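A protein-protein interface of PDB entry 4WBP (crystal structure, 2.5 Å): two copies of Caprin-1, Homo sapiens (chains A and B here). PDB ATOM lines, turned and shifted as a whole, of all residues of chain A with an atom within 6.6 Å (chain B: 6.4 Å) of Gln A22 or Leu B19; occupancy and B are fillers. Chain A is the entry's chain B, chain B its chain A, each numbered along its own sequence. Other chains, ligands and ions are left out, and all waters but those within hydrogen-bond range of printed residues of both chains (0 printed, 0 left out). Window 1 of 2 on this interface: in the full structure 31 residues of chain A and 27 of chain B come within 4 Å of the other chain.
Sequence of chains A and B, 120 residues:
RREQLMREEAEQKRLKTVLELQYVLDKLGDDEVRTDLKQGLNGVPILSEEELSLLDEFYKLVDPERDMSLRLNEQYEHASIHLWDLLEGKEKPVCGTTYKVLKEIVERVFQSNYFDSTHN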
ATOM      1  N   LEU A  15      11.939 -22.369 -18.513  1.00  0.00           N
ATOM      2  CA  LEU A  15      12.191 -23.516 -19.383  1.00  0.00           C
ATOM      3  C   LEU A  15      11.279 -24.681 -19.014  1.00  0.00           C
ATOM      4  O   LEU A  15      10.685 -25.317 -19.888  1.00  0.00           O
ATOM      5  CB  LEU A  15      13.652 -23.963 -19.306  1.00  0.00           C
ATOM      6  CG  LEU A  15      14.698 -23.132 -20.049  1.00  0.00           C
ATOM      7  CD1 LEU A  15      16.065 -23.796 -19.958  1.00  0.00           C
ATOM      8  CD2 LEU A  15      14.287 -22.930 -21.501  1.00  0.00           C
ATOM      9  N   THR A  17       8.400 -24.590 -17.498  1.00  0.00           N
ATOM     10  CA  THR A  17       7.039 -24.234 -17.885  1.00  0.00           C
ATOM     11  C   THR A  17       6.830 -24.419 -19.387  1.00  0.00           C
ATOM     12  O   THR A  17       5.780 -24.893 -19.823  1.00  0.00           O
ATOM     13  CB  THR A  17       6.701 -22.788 -17.479  1.00  0.00           C
ATOM     14  OG1 THR A  17       6.845 -22.651 -16.060  1.00  0.00           O
ATOM     15  CG2 THR A  17       5.274 -22.436 -17.870  1.00  0.00           C
ATOM     16  N   VAL A  18       7.838 -24.050 -20.174  1.00  0.00           N
ATOM     17  CA  VAL A  18       7.781 -24.235 -21.617  1.00  0.00           C
ATOM     18  C   VAL A  18       7.644 -25.714 -21.958  1.00  0.00           C
ATOM     19  O   VAL A  18       6.811 -26.090 -22.779  1.00  0.00           O
ATOM     20  CB  VAL A  18       9.025 -23.654 -22.322  1.00  0.00           C
ATOM     21  CG1 VAL A  18       9.086 -24.120 -23.775  1.00  0.00           C
ATOM     22  CG2 VAL A  18       9.020 -22.133 -22.238  1.00  0.00           C
ATOM     23  N   LEU A  19       8.460 -26.551 -21.322  1.00  0.00           N
ATOM     24  CA  LEU A  19       8.383 -27.995 -21.536  1.00  0.00           C
ATOM     25  C   LEU A  19       7.001 -28.556 -21.197  1.00  0.00           C
ATOM     26  O   LEU A  19       6.426 -29.328 -21.973  1.00  0.00           O
ATOM     27  CB  LEU A  19       9.466 -28.716 -20.733  1.00  0.00           C
ATOM     28  CG  LEU A  19      10.899 -28.327 -21.102  1.00  0.00           C
ATOM     29  CD1 LEU A  19      11.895 -28.991 -20.163  1.00  0.00           C
ATOM     30  CD2 LEU A  19      11.198 -28.676 -22.555  1.00  0.00           C
ATOM     31  N   GLU A  20       6.463 -28.148 -20.049  1.00  0.00           N
ATOM     32  CA  GLU A  20       5.131 -28.587 -19.642  1.00  0.00           C
ATOM     33  C   GLU A  20       4.086 -28.172 -20.676  1.00  0.00           C
ATOM     34  O   GLU A  20       3.206 -28.958 -21.049  1.00  0.00           O
ATOM     35  CB  GLU A  20       4.770 -28.001 -18.275  1.00  0.00           C
ATOM     36  CG  GLU A  20       5.699 -28.425 -17.149  1.00  0.00           C
ATOM     37  CD  GLU A  20       5.556 -27.553 -15.914  1.00  0.00           C
ATOM     38  OE1 GLU A  20       4.607 -26.743 -15.864  1.00  0.00           O
ATOM     39  OE2 GLU A  20       6.399 -27.670 -14.998  1.00  0.00           O
ATOM     40  N   LEU A  21       4.206 -26.937 -21.151  1.00  0.00           N
ATOM     41  CA  LEU A  21       3.305 -26.409 -22.167  1.00  0.00           C
ATOM     42  C   LEU A  21       3.388 -27.205 -23.465  1.00  0.00           C
ATOM     43  O   LEU A  21       2.371 -27.487 -24.092  1.00  0.00           O
ATOM     44  CB  LEU A  21       3.613 -24.938 -22.438  1.00  0.00           C
ATOM     45  CG  LEU A  21       2.815 -24.311 -23.580  1.00  0.00           C
ATOM     46  CD1 LEU A  21       1.344 -24.204 -23.209  1.00  0.00           C
ATOM     47  CD2 LEU A  21       3.383 -22.956 -23.941  1.00  0.00           C
ATOM     48  N   GLN A  22       4.605 -27.559 -23.864  1.00  0.00           N
ATOM     49  CA  GLN A  22       4.817 -28.340 -25.073  1.00  0.00           C
ATOM     50  C   GLN A  22       4.135 -29.688 -24.925  1.00  0.00           C
ATOM     51  O   GLN A  22       3.507 -30.180 -25.862  1.00  0.00           O
ATOM     52  CB  GLN A  22       6.309 -28.547 -25.334  1.00  0.00           C
ATOM     53  CG  GLN A  22       7.040 -27.322 -25.845  1.00  0.00           C
ATOM     54  CD  GLN A  22       8.526 -27.567 -26.003  1.00  0.00           C
ATOM     55  OE1 GLN A  22       9.127 -28.314 -25.233  1.00  0.00           O
ATOM     56  NE2 GLN A  22       9.123 -26.949 -27.012  1.00  0.00           N
ATOM     57  N   TYR A  23       4.257 -30.273 -23.736  1.00  0.00           N
ATOM     58  CA  TYR A  23       3.581 -31.531 -23.442  1.00  0.00           C
ATOM     59  C   TYR A  23       2.067 -31.386 -23.611  1.00  0.00           C
ATOM     60  O   TYR A  23       1.434 -32.183 -24.307  1.00  0.00           O
ATOM     61  CB  TYR A  23       3.912 -32.009 -22.028  1.00  0.00           C
ATOM     62  CG  TYR A  23       3.280 -33.336 -21.666  1.00  0.00           C
ATOM     63  CD1 TYR A  23       3.877 -34.531 -22.044  1.00  0.00           C
ATOM     64  CD2 TYR A  23       2.086 -33.395 -20.958  1.00  0.00           C
ATOM     65  CE1 TYR A  23       3.311 -35.748 -21.721  1.00  0.00           C
ATOM     66  CE2 TYR A  23       1.510 -34.610 -20.630  1.00  0.00           C
ATOM     67  CZ  TYR A  23       2.129 -35.782 -21.014  1.00  0.00           C
ATOM     68  OH  TYR A  23       1.564 -36.996 -20.693  1.00  0.00           O
ATOM     69  N   VAL A  24       1.493 -30.367 -22.975  1.00  0.00           N
ATOM     70  CA  VAL A  24       0.047 -30.143 -23.044  1.00  0.00           C
ATOM     71  C   VAL A  24      -0.460 -29.923 -24.469  1.00  0.00           C
ATOM     72  O   VAL A  24      -1.408 -30.575 -24.907  1.00  0.00           O
ATOM     73  CB  VAL A  24      -0.386 -28.952 -22.168  1.00  0.00           C
ATOM     74  CG1 VAL A  24      -1.822 -28.560 -22.477  1.00  0.00           C
ATOM     75  CG2 VAL A  24      -0.226 -29.294 -20.698  1.00  0.00           C
ATOM     76  N   LEU A  25       0.177 -29.004 -25.187  1.00  0.00           N
ATOM     77  CA  LEU A  25      -0.208 -28.699 -26.559  1.00  0.00           C
ATOM     78  C   LEU A  25      -0.069 -29.940 -27.429  1.00  0.00           C
ATOM     79  O   LEU A  25      -0.848 -30.155 -28.356  1.00  0.00           O
ATOM     80  CB  LEU A  25       0.640 -27.555 -27.120  1.00  0.00           C
ATOM     81  CG  LEU A  25       0.453 -26.189 -26.456  1.00  0.00           C
ATOM     82  CD1 LEU A  25       1.375 -25.151 -27.079  1.00  0.00           C
ATOM     83  CD2 LEU A  25      -0.998 -25.738 -26.534  1.00  0.00           C
ATOM     84  N   ASP A  26       0.929 -30.759 -27.117  1.00  0.00           N
ATOM     85  CA  ASP A  26       1.144 -32.005 -27.838  1.00  0.00           C
ATOM     86  C   ASP A  26      -0.028 -32.952 -27.576  1.00  0.00           C
ATOM     87  O   ASP A  26      -0.498 -33.637 -28.485  1.00  0.00           O
ATOM     88  CB  ASP A  26       2.468 -32.636 -27.393  1.00  0.00           C
ATOM     89  CG  ASP A  26       2.877 -33.824 -28.243  1.00  0.00           C
ATOM     90  OD1 ASP A  26       2.082 -34.774 -28.394  1.00  0.00           O
ATOM     91  OD2 ASP A  26       4.014 -33.803 -28.761  1.00  0.00           O
ATOM     92  N   LYS A  27      -0.505 -32.976 -26.334  1.00  0.00           N
ATOM     93  CA  LYS A  27      -1.632 -33.831 -25.964  1.00  0.00           C
ATOM     94  C   LYS A  27      -2.967 -33.320 -26.500  1.00  0.00           C
ATOM     95  O   LYS A  27      -3.924 -34.084 -26.628  1.00  0.00           O
ATOM     96  CB  LYS A  27      -1.718 -33.961 -24.442  1.00  0.00           C
ATOM     97  CG  LYS A  27      -0.584 -34.754 -23.823  1.00  0.00           C
ATOM     98  CD  LYS A  27      -0.585 -36.189 -24.312  1.00  0.00           C
ATOM     99  CE  LYS A  27       0.702 -36.895 -23.931  1.00  0.00           C
ATOM    100  NZ  LYS A  27       0.657 -38.347 -24.250  1.00  0.00           N
ATOM    101  N   TYR A  59      -0.561 -23.066 -30.979  1.00  0.00           N
ATOM    102  CA  TYR A  59       0.250 -24.247 -31.238  1.00  0.00           C
ATOM    103  C   TYR A  59       0.871 -24.174 -32.626  1.00  0.00           C
ATOM    104  O   TYR A  59       2.016 -24.589 -32.821  1.00  0.00           O
ATOM    105  CB  TYR A  59      -0.580 -25.522 -31.091  1.00  0.00           C
ATOM    106  CG  TYR A  59       0.141 -26.769 -31.543  1.00  0.00           C
ATOM    107  CD1 TYR A  59       1.200 -27.289 -30.810  1.00  0.00           C
ATOM    108  CD2 TYR A  59      -0.233 -27.424 -32.710  1.00  0.00           C
ATOM    109  CE1 TYR A  59       1.863 -28.433 -31.224  1.00  0.00           C
ATOM    110  CE2 TYR A  59       0.423 -28.564 -33.132  1.00  0.00           C
ATOM    111  CZ  TYR A  59       1.470 -29.065 -32.387  1.00  0.00           C
ATOM    112  OH  TYR A  59       2.123 -30.200 -32.808  1.00  0.00           O
ATOM    113  N   VAL A  62       3.922 -21.853 -32.228  1.00  0.00           N
ATOM    114  CA  VAL A  62       5.077 -22.278 -31.432  1.00  0.00           C
ATOM    115  C   VAL A  62       5.713 -23.601 -31.856  1.00  0.00           C
ATOM    116  O   VAL A  62       6.827 -23.914 -31.442  1.00  0.00           O
ATOM    117  CB  VAL A  62       4.755 -22.314 -29.930  1.00  0.00           C
ATOM    118  CG1 VAL A  62       4.533 -20.905 -29.420  1.00  0.00           C
ATOM    119  CG2 VAL A  62       3.544 -23.198 -29.665  1.00  0.00           C
ATOM    120  N   LEU A  72      17.892 -22.884 -40.153  1.00  0.00           N
ATOM    121  CA  LEU A  72      17.458 -23.449 -38.877  1.00  0.00           C
ATOM    122  C   LEU A  72      17.466 -22.426 -37.740  1.00  0.00           C
ATOM    123  O   LEU A  72      16.574 -22.428 -36.891  1.00  0.00           O
ATOM    124  CB  LEU A  72      18.308 -24.664 -38.497  1.00  0.00           C
ATOM    125  CG  LEU A  72      17.958 -25.284 -37.141  1.00  0.00           C
ATOM    126  CD1 LEU A  72      16.526 -25.805 -37.145  1.00  0.00           C
ATOM    127  CD2 LEU A  72      18.935 -26.384 -36.762  1.00  0.00           C
ATOM    128  N   TYR A  76      12.869 -20.597 -35.478  1.00  0.00           N
ATOM    129  CA  TYR A  76      12.198 -20.513 -34.183  1.00  0.00           C
ATOM    130  C   TYR A  76      12.294 -19.158 -33.488  1.00  0.00           C
ATOM    131  O   TYR A  76      12.024 -19.051 -32.292  1.00  0.00           O
ATOM    132  CB  TYR A  76      12.693 -21.633 -33.271  1.00  0.00           C
ATOM    133  CG  TYR A  76      12.303 -22.998 -33.778  1.00  0.00           C
ATOM    134  CD1 TYR A  76      11.016 -23.489 -33.596  1.00  0.00           C
ATOM    135  CD2 TYR A  76      13.214 -23.786 -34.465  1.00  0.00           C
ATOM    136  CE1 TYR A  76      10.657 -24.737 -34.069  1.00  0.00           C
ATOM    137  CE2 TYR A  76      12.865 -25.033 -34.941  1.00  0.00           C
ATOM    138  CZ  TYR A  76      11.586 -25.503 -34.742  1.00  0.00           C
ATOM    139  OH  TYR A  76      11.244 -26.748 -35.220  1.00  0.00           O
ATOM    140  N   GLU A  77      12.684 -18.133 -34.238  1.00  0.00           N
ATOM    141  CA  GLU A  77      12.721 -16.772 -33.718  1.00  0.00           C
ATOM    142  C   GLU A  77      11.339 -16.353 -33.224  1.00  0.00           C
ATOM    143  O   GLU A  77      11.155 -16.014 -32.043  1.00  0.00           O
ATOM    144  CB  GLU A  77      13.174 -15.814 -34.822  1.00  0.00           C
ATOM    145  CG  GLU A  77      13.177 -14.342 -34.436  1.00  0.00           C
ATOM    146  CD  GLU A  77      14.470 -13.905 -33.777  1.00  0.00           C
ATOM    147  OE1 GLU A  77      15.467 -14.653 -33.867  1.00  0.00           O
ATOM    148  OE2 GLU A  77      14.496 -12.805 -33.186  1.00  0.00           O
ATOM    149  N   HIS A  78      10.360 -16.396 -34.123  1.00  0.00           N
ATOM    150  CA  HIS A  78       9.011 -15.984 -33.766  1.00  0.00           C
ATOM    151  C   HIS A  78       8.438 -16.912 -32.706  1.00  0.00           C
ATOM    152  O   HIS A  78       7.726 -16.465 -31.824  1.00  0.00           O
ATOM    153  CB  HIS A  78       8.072 -15.923 -34.975  1.00  0.00           C
ATOM    154  CG  HIS A  78       8.430 -14.860 -35.965  1.00  0.00           C
ATOM    155  ND1 HIS A  78       8.037 -14.919 -37.288  1.00  0.00           N
ATOM    156  CD2 HIS A  78       9.192 -13.748 -35.854  1.00  0.00           C
ATOM    157  CE1 HIS A  78       8.516 -13.877 -37.935  1.00  0.00           C
ATOM    158  NE2 HIS A  78       9.226 -13.147 -37.088  1.00  0.00           N
ATOM    159  N   ALA A  79       8.749 -18.204 -32.797  1.00  0.00           N
ATOM    160  CA  ALA A  79       8.299 -19.165 -31.791  1.00  0.00           C
ATOM    161  C   ALA A  79       8.818 -18.802 -30.402  1.00  0.00           C
ATOM    162  O   ALA A  79       8.055 -18.779 -29.430  1.00  0.00           O
ATOM    163  CB  ALA A  79       8.731 -20.570 -32.164  1.00  0.00           C
ATOM    164  N   SER A  80      10.116 -18.525 -30.315  1.00  0.00           N
ATOM    165  CA  SER A  80      10.731 -18.111 -29.058  1.00  0.00           C
ATOM    166  C   SER A  80      10.068 -16.856 -28.502  1.00  0.00           C
ATOM    167  O   SER A  80       9.771 -16.780 -27.302  1.00  0.00           O
ATOM    168  CB  SER A  80      12.231 -17.876 -29.242  1.00  0.00           C
ATOM    169  OG  SER A  80      12.475 -16.757 -30.076  1.00  0.00           O
ATOM    170  N   ILE A  81       9.811 -15.883 -29.372  1.00  0.00           N
ATOM    171  CA  ILE A  81       9.168 -14.652 -28.915  1.00  0.00           C
ATOM    172  C   ILE A  81       7.726 -14.904 -28.464  1.00  0.00           C
ATOM    173  O   ILE A  81       7.253 -14.294 -27.506  1.00  0.00           O
ATOM    174  CB  ILE A  81       9.189 -13.546 -29.991  1.00  0.00           C
ATOM    175  CG1 ILE A  81      10.615 -13.313 -30.487  1.00  0.00           C
ATOM    176  CG2 ILE A  81       8.601 -12.253 -29.444  1.00  0.00           C
ATOM    177  CD1 ILE A  81      11.579 -12.944 -29.392  1.00  0.00           C
ATOM    178  N   LEU A  83       6.504 -17.744 -27.182  1.00  0.00           N
ATOM    179  CA  LEU A  83       6.530 -18.433 -25.902  1.00  0.00           C
ATOM    180  C   LEU A  83       6.892 -17.467 -24.785  1.00  0.00           C
ATOM    181  O   LEU A  83       6.269 -17.477 -23.720  1.00  0.00           O
ATOM    182  CB  LEU A  83       7.517 -19.600 -25.931  1.00  0.00           C
ATOM    183  CG  LEU A  83       7.087 -20.831 -26.732  1.00  0.00           C
ATOM    184  CD1 LEU A  83       8.277 -21.728 -27.027  1.00  0.00           C
ATOM    185  CD2 LEU A  83       6.007 -21.600 -25.995  1.00  0.00           C
ATOM    186  N   PHE A 110      -3.556 -26.210 -16.679  1.00  0.00           N
ATOM    187  CA  PHE A 110      -2.567 -26.686 -15.717  1.00  0.00           C
ATOM    188  C   PHE A 110      -3.196 -26.994 -14.360  1.00  0.00           C
ATOM    189  O   PHE A 110      -2.908 -28.024 -13.753  1.00  0.00           O
ATOM    190  CB  PHE A 110      -1.470 -25.635 -15.515  1.00  0.00           C
ATOM    191  CG  PHE A 110      -0.423 -25.617 -16.594  1.00  0.00           C
ATOM    192  CD1 PHE A 110      -0.331 -26.643 -17.517  1.00  0.00           C
ATOM    193  CD2 PHE A 110       0.489 -24.573 -16.667  1.00  0.00           C
ATOM    194  CE1 PHE A 110       0.640 -26.622 -18.503  1.00  0.00           C
ATOM    195  CE2 PHE A 110       1.463 -24.548 -17.647  1.00  0.00           C
ATOM    196  CZ  PHE A 110       1.539 -25.574 -18.567  1.00  0.00           C
ATOM    197  N   ARG B  14      18.100 -17.841 -25.937  1.00  0.00           N
ATOM    198  CA  ARG B  14      18.296 -19.147 -25.312  1.00  0.00           C
ATOM    199  C   ARG B  14      17.111 -20.092 -25.561  1.00  0.00           C
ATOM    200  O   ARG B  14      17.293 -21.276 -25.866  1.00  0.00           O
ATOM    201  CB  ARG B  14      18.575 -18.995 -23.820  1.00  0.00           C
ATOM    202  CG  ARG B  14      20.045 -19.112 -23.485  1.00  0.00           C
ATOM    203  CD  ARG B  14      20.422 -18.254 -22.299  1.00  0.00           C
ATOM    204  NE  ARG B  14      21.831 -18.422 -21.965  1.00  0.00           N
ATOM    205  CZ  ARG B  14      22.287 -19.332 -21.112  1.00  0.00           C
ATOM    206  NH1 ARG B  14      21.440 -20.150 -20.502  1.00  0.00           N
ATOM    207  NH2 ARG B  14      23.586 -19.422 -20.866  1.00  0.00           N
ATOM    208  N   LEU B  15      15.902 -19.556 -25.432  1.00  0.00           N
ATOM    209  CA  LEU B  15      14.680 -20.300 -25.725  1.00  0.00           C
ATOM    210  C   LEU B  15      14.691 -20.816 -27.170  1.00  0.00           C
ATOM    211  O   LEU B  15      14.353 -21.977 -27.441  1.00  0.00           O
ATOM    212  CB  LEU B  15      13.470 -19.398 -25.473  1.00  0.00           C
ATOM    213  CG  LEU B  15      12.070 -19.995 -25.349  1.00  0.00           C
ATOM    214  CD1 LEU B  15      12.120 -21.379 -24.725  1.00  0.00           C
ATOM    215  CD2 LEU B  15      11.205 -19.065 -24.511  1.00  0.00           C
ATOM    216  N   LYS B  16      15.097 -19.942 -28.087  1.00  0.00           N
ATOM    217  CA  LYS B  16      15.181 -20.266 -29.504  1.00  0.00           C
ATOM    218  C   LYS B  16      16.164 -21.406 -29.720  1.00  0.00           C
ATOM    219  O   LYS B  16      15.897 -22.341 -30.485  1.00  0.00           O
ATOM    220  CB  LYS B  16      15.631 -19.034 -30.294  1.00  0.00           C
ATOM    221  CG  LYS B  16      15.789 -19.264 -31.789  1.00  0.00           C
ATOM    222  CD  LYS B  16      16.093 -17.960 -32.516  1.00  0.00           C
ATOM    223  CE  LYS B  16      17.582 -17.644 -32.519  1.00  0.00           C
ATOM    224  NZ  LYS B  16      18.356 -18.530 -33.434  1.00  0.00           N
ATOM    225  N   THR B  17      17.294 -21.330 -29.021  1.00  0.00           N
ATOM    226  CA  THR B  17      18.316 -22.363 -29.107  1.00  0.00           C
ATOM    227  C   THR B  17      17.750 -23.696 -28.627  1.00  0.00           C
ATOM    228  O   THR B  17      18.016 -24.744 -29.219  1.00  0.00           O
ATOM    229  CB  THR B  17      19.557 -21.997 -28.272  1.00  0.00           C
ATOM    230  OG1 THR B  17      20.092 -20.750 -28.732  1.00  0.00           O
ATOM    231  CG2 THR B  17      20.626 -23.076 -28.391  1.00  0.00           C
ATOM    232  N   VAL B  18      16.953 -23.644 -27.564  1.00  0.00           N
ATOM    233  CA  VAL B  18      16.299 -24.843 -27.048  1.00  0.00           C
ATOM    234  C   VAL B  18      15.366 -25.462 -28.090  1.00  0.00           C
ATOM    235  O   VAL B  18      15.400 -26.675 -28.319  1.00  0.00           O
ATOM    236  CB  VAL B  18      15.515 -24.553 -25.752  1.00  0.00           C
ATOM    237  CG1 VAL B  18      14.599 -25.721 -25.404  1.00  0.00           C
ATOM    238  CG2 VAL B  18      16.475 -24.253 -24.608  1.00  0.00           C
ATOM    239  N   LEU B  19      14.540 -24.631 -28.719  1.00  0.00           N
ATOM    240  CA  LEU B  19      13.637 -25.113 -29.766  1.00  0.00           C
ATOM    241  C   LEU B  19      14.390 -25.772 -30.927  1.00  0.00           C
ATOM    242  O   LEU B  19      14.021 -26.861 -31.391  1.00  0.00           O
ATOM    243  CB  LEU B  19      12.750 -23.976 -30.274  1.00  0.00           C
ATOM    244  CG  LEU B  19      11.844 -23.354 -29.210  1.00  0.00           C
ATOM    245  CD1 LEU B  19      11.103 -22.142 -29.759  1.00  0.00           C
ATOM    246  CD2 LEU B  19      10.866 -24.392 -28.685  1.00  0.00           C
ATOM    247  N   GLU B  20      15.449 -25.110 -31.385  1.00  0.00           N
ATOM    248  CA  GLU B  20      16.282 -25.650 -32.456  1.00  0.00           C
ATOM    249  C   GLU B  20      16.900 -26.997 -32.067  1.00  0.00           C
ATOM    250  O   GLU B  20      16.932 -27.938 -32.870  1.00  0.00           O
ATOM    251  CB  GLU B  20      17.354 -24.635 -32.863  1.00  0.00           C
ATOM    252  CG  GLU B  20      16.771 -23.337 -33.419  1.00  0.00           C
ATOM    253  CD  GLU B  20      17.775 -22.198 -33.471  1.00  0.00           C
ATOM    254  OE1 GLU B  20      18.976 -22.446 -33.236  1.00  0.00           O
ATOM    255  OE2 GLU B  20      17.361 -21.055 -33.765  1.00  0.00           O
ATOM    256  N   LEU B  21      17.378 -27.086 -30.828  1.00  0.00           N
ATOM    257  CA  LEU B  21      17.938 -28.332 -30.323  1.00  0.00           C
ATOM    258  C   LEU B  21      16.887 -29.434 -30.319  1.00  0.00           C
ATOM    259  O   LEU B  21      17.177 -30.571 -30.673  1.00  0.00           O
ATOM    260  CB  LEU B  21      18.501 -28.159 -28.913  1.00  0.00           C
ATOM    261  CG  LEU B  21      18.974 -29.469 -28.272  1.00  0.00           C
ATOM    262  CD1 LEU B  21      20.201 -30.016 -28.990  1.00  0.00           C
ATOM    263  CD2 LEU B  21      19.243 -29.299 -26.786  1.00  0.00           C
ATOM    264  N   GLN B  22      15.667 -29.092 -29.916  1.00  0.00           N
ATOM    265  CA  GLN B  22      14.583 -30.065 -29.882  1.00  0.00           C
ATOM    266  C   GLN B  22      14.307 -30.585 -31.287  1.00  0.00           C
ATOM    267  O   GLN B  22      14.098 -31.789 -31.488  1.00  0.00           O
ATOM    268  CB  GLN B  22      13.324 -29.450 -29.269  1.00  0.00           C
ATOM    269  CG  GLN B  22      13.414 -29.256 -27.757  1.00  0.00           C
ATOM    270  CD  GLN B  22      12.195 -28.568 -27.180  1.00  0.00           C
ATOM    271  OE1 GLN B  22      11.581 -27.719 -27.825  1.00  0.00           O
ATOM    272  NE2 GLN B  22      11.844 -28.925 -25.953  1.00  0.00           N
ATOM    273  N   TYR B  23      14.330 -29.675 -32.259  1.00  0.00           N
ATOM    274  CA  TYR B  23      14.183 -30.060 -33.661  1.00  0.00           C
ATOM    275  C   TYR B  23      15.261 -31.051 -34.100  1.00  0.00           C
ATOM    276  O   TYR B  23      14.959 -32.124 -34.646  1.00  0.00           O
ATOM    277  CB  TYR B  23      14.214 -28.826 -34.567  1.00  0.00           C
ATOM    278  CG  TYR B  23      14.107 -29.161 -36.038  1.00  0.00           C
ATOM    279  CD1 TYR B  23      12.875 -29.400 -36.632  1.00  0.00           C
ATOM    280  CD2 TYR B  23      15.244 -29.242 -36.834  1.00  0.00           C
ATOM    281  CE1 TYR B  23      12.777 -29.711 -37.976  1.00  0.00           C
ATOM    282  CE2 TYR B  23      15.156 -29.551 -38.178  1.00  0.00           C
ATOM    283  CZ  TYR B  23      13.921 -29.785 -38.744  1.00  0.00           C
ATOM    284  OH  TYR B  23      13.834 -30.094 -40.083  1.00  0.00           O
ATOM    285  N   VAL B  24      16.517 -30.688 -33.847  1.00  0.00           N
ATOM    286  CA  VAL B  24      17.649 -31.521 -34.238  1.00  0.00           C
ATOM    287  C   VAL B  24      17.576 -32.907 -33.597  1.00  0.00           C
ATOM    288  O   VAL B  24      17.703 -33.925 -34.280  1.00  0.00           O
ATOM    289  CB  VAL B  24      18.989 -30.854 -33.875  1.00  0.00           C
ATOM    290  CG1 VAL B  24      20.137 -31.837 -34.046  1.00  0.00           C
ATOM    291  CG2 VAL B  24      19.211 -29.616 -34.732  1.00  0.00           C
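The side-chain amide oxygen of Gln B22 lies within hydrogen-bond range of the side-chain amide nitrogen of Gln A22 (2.7 Å).
The side-chain amino group (NZ) of Lys B16 is in salt-bridge range of the side-chain carboxylate (OE2) of Glu B20, 2.7 Å away.
O of Tyr A76 sits at hydrogen-bond distance from OG of Ser A80 (3.2 Å).
The side-chain hydroxyl (OG) of Ser A80 sits at hydrogen-bond distance from the backbone carbonyl oxygen (O) of Glu A77, at 2.5 Å.
Leu A19 touches Gln B22.
Gln A22 touches Leu B19.
Tyr A76 touches Leu B19.
Tyr A76 touches Glu B20.
Ala A79 touches Leu B19 (CB to CD1, 3.7 Å).
Ser A80 touches Leu B15.
CB of Ser A80 touches N of Lys B16, at 3.7 Å.
Ser A80 touches Leu B19 (N to CD1, 3.8 Å).
CB of Leu A83 touches CD2 of Leu B15, 3.99 Å away.
Leu B19 touches Leu A83.
Gln A22 touches two residues of chain B.
Leu A25 touches none of the printed residues of chain B.
Printed residues of chain B within 4 Å of Glu A77: Lys B16 (3.6 Å).
Printed residues of chain B within 4 Å of Ala A79: Leu B19 (3.7 Å).
Of the printed residues of chain B, Leu A83 touches Leu B15 (3.99 Å) and Leu B19 (3.95 Å).
Arg B14 touches none of the printed residues of chain A.
Leu B19 touches just these residues of chain A: Gln A22 (3.5 Å), Tyr A76 (3.7 Å), Ala A79 (3.7 Å), Ser A80 (3.8 Å) and Leu A83 (3.95 Å).
Printed residues of chain A within 4 Å of Val B24: Leu A72.
The nearest residue of chain B that does not touch Gln A22 is Val B18 (5.8 Å).
The nearest residue of chain A that does not touch Leu B19 is Val A62 (4.9 Å).
The nearest printed residue of chain B that does not touch Ser A80 is Thr B17 (6.1 Å).
Printed residues of chain B that touch a printed residue of chain A: Leu B15, Lys B16, Leu B19, Glu B20, Gln B22, Tyr B23 and Val B24.
Hydrophobic or aromatic side chains of chain B within 4 Å of the printed part of chain A: Leu B15, Leu B19, Tyr B23 and Val B24.
Hydrophobic or aromatic side chains of chain A that line the printed part of chain B: Leu A19, Leu A72, Tyr A76, Ala A79 and Leu A83.
Among the printed residues, 17 pairs touch across the chains.
Leu A19 touches Gln B22, and with the chains exchanged Gln A22 touches Leu B19.
Gln B22 touches its own counterpart, Gln A22.
Positions printed for both chains: 15, 17, 18, 19, 20, 21, 22, 23 and 24.
Of the 17 pairs that touch across the chains among the printed residues, 3 have their exchanged pair printed and touching as well.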
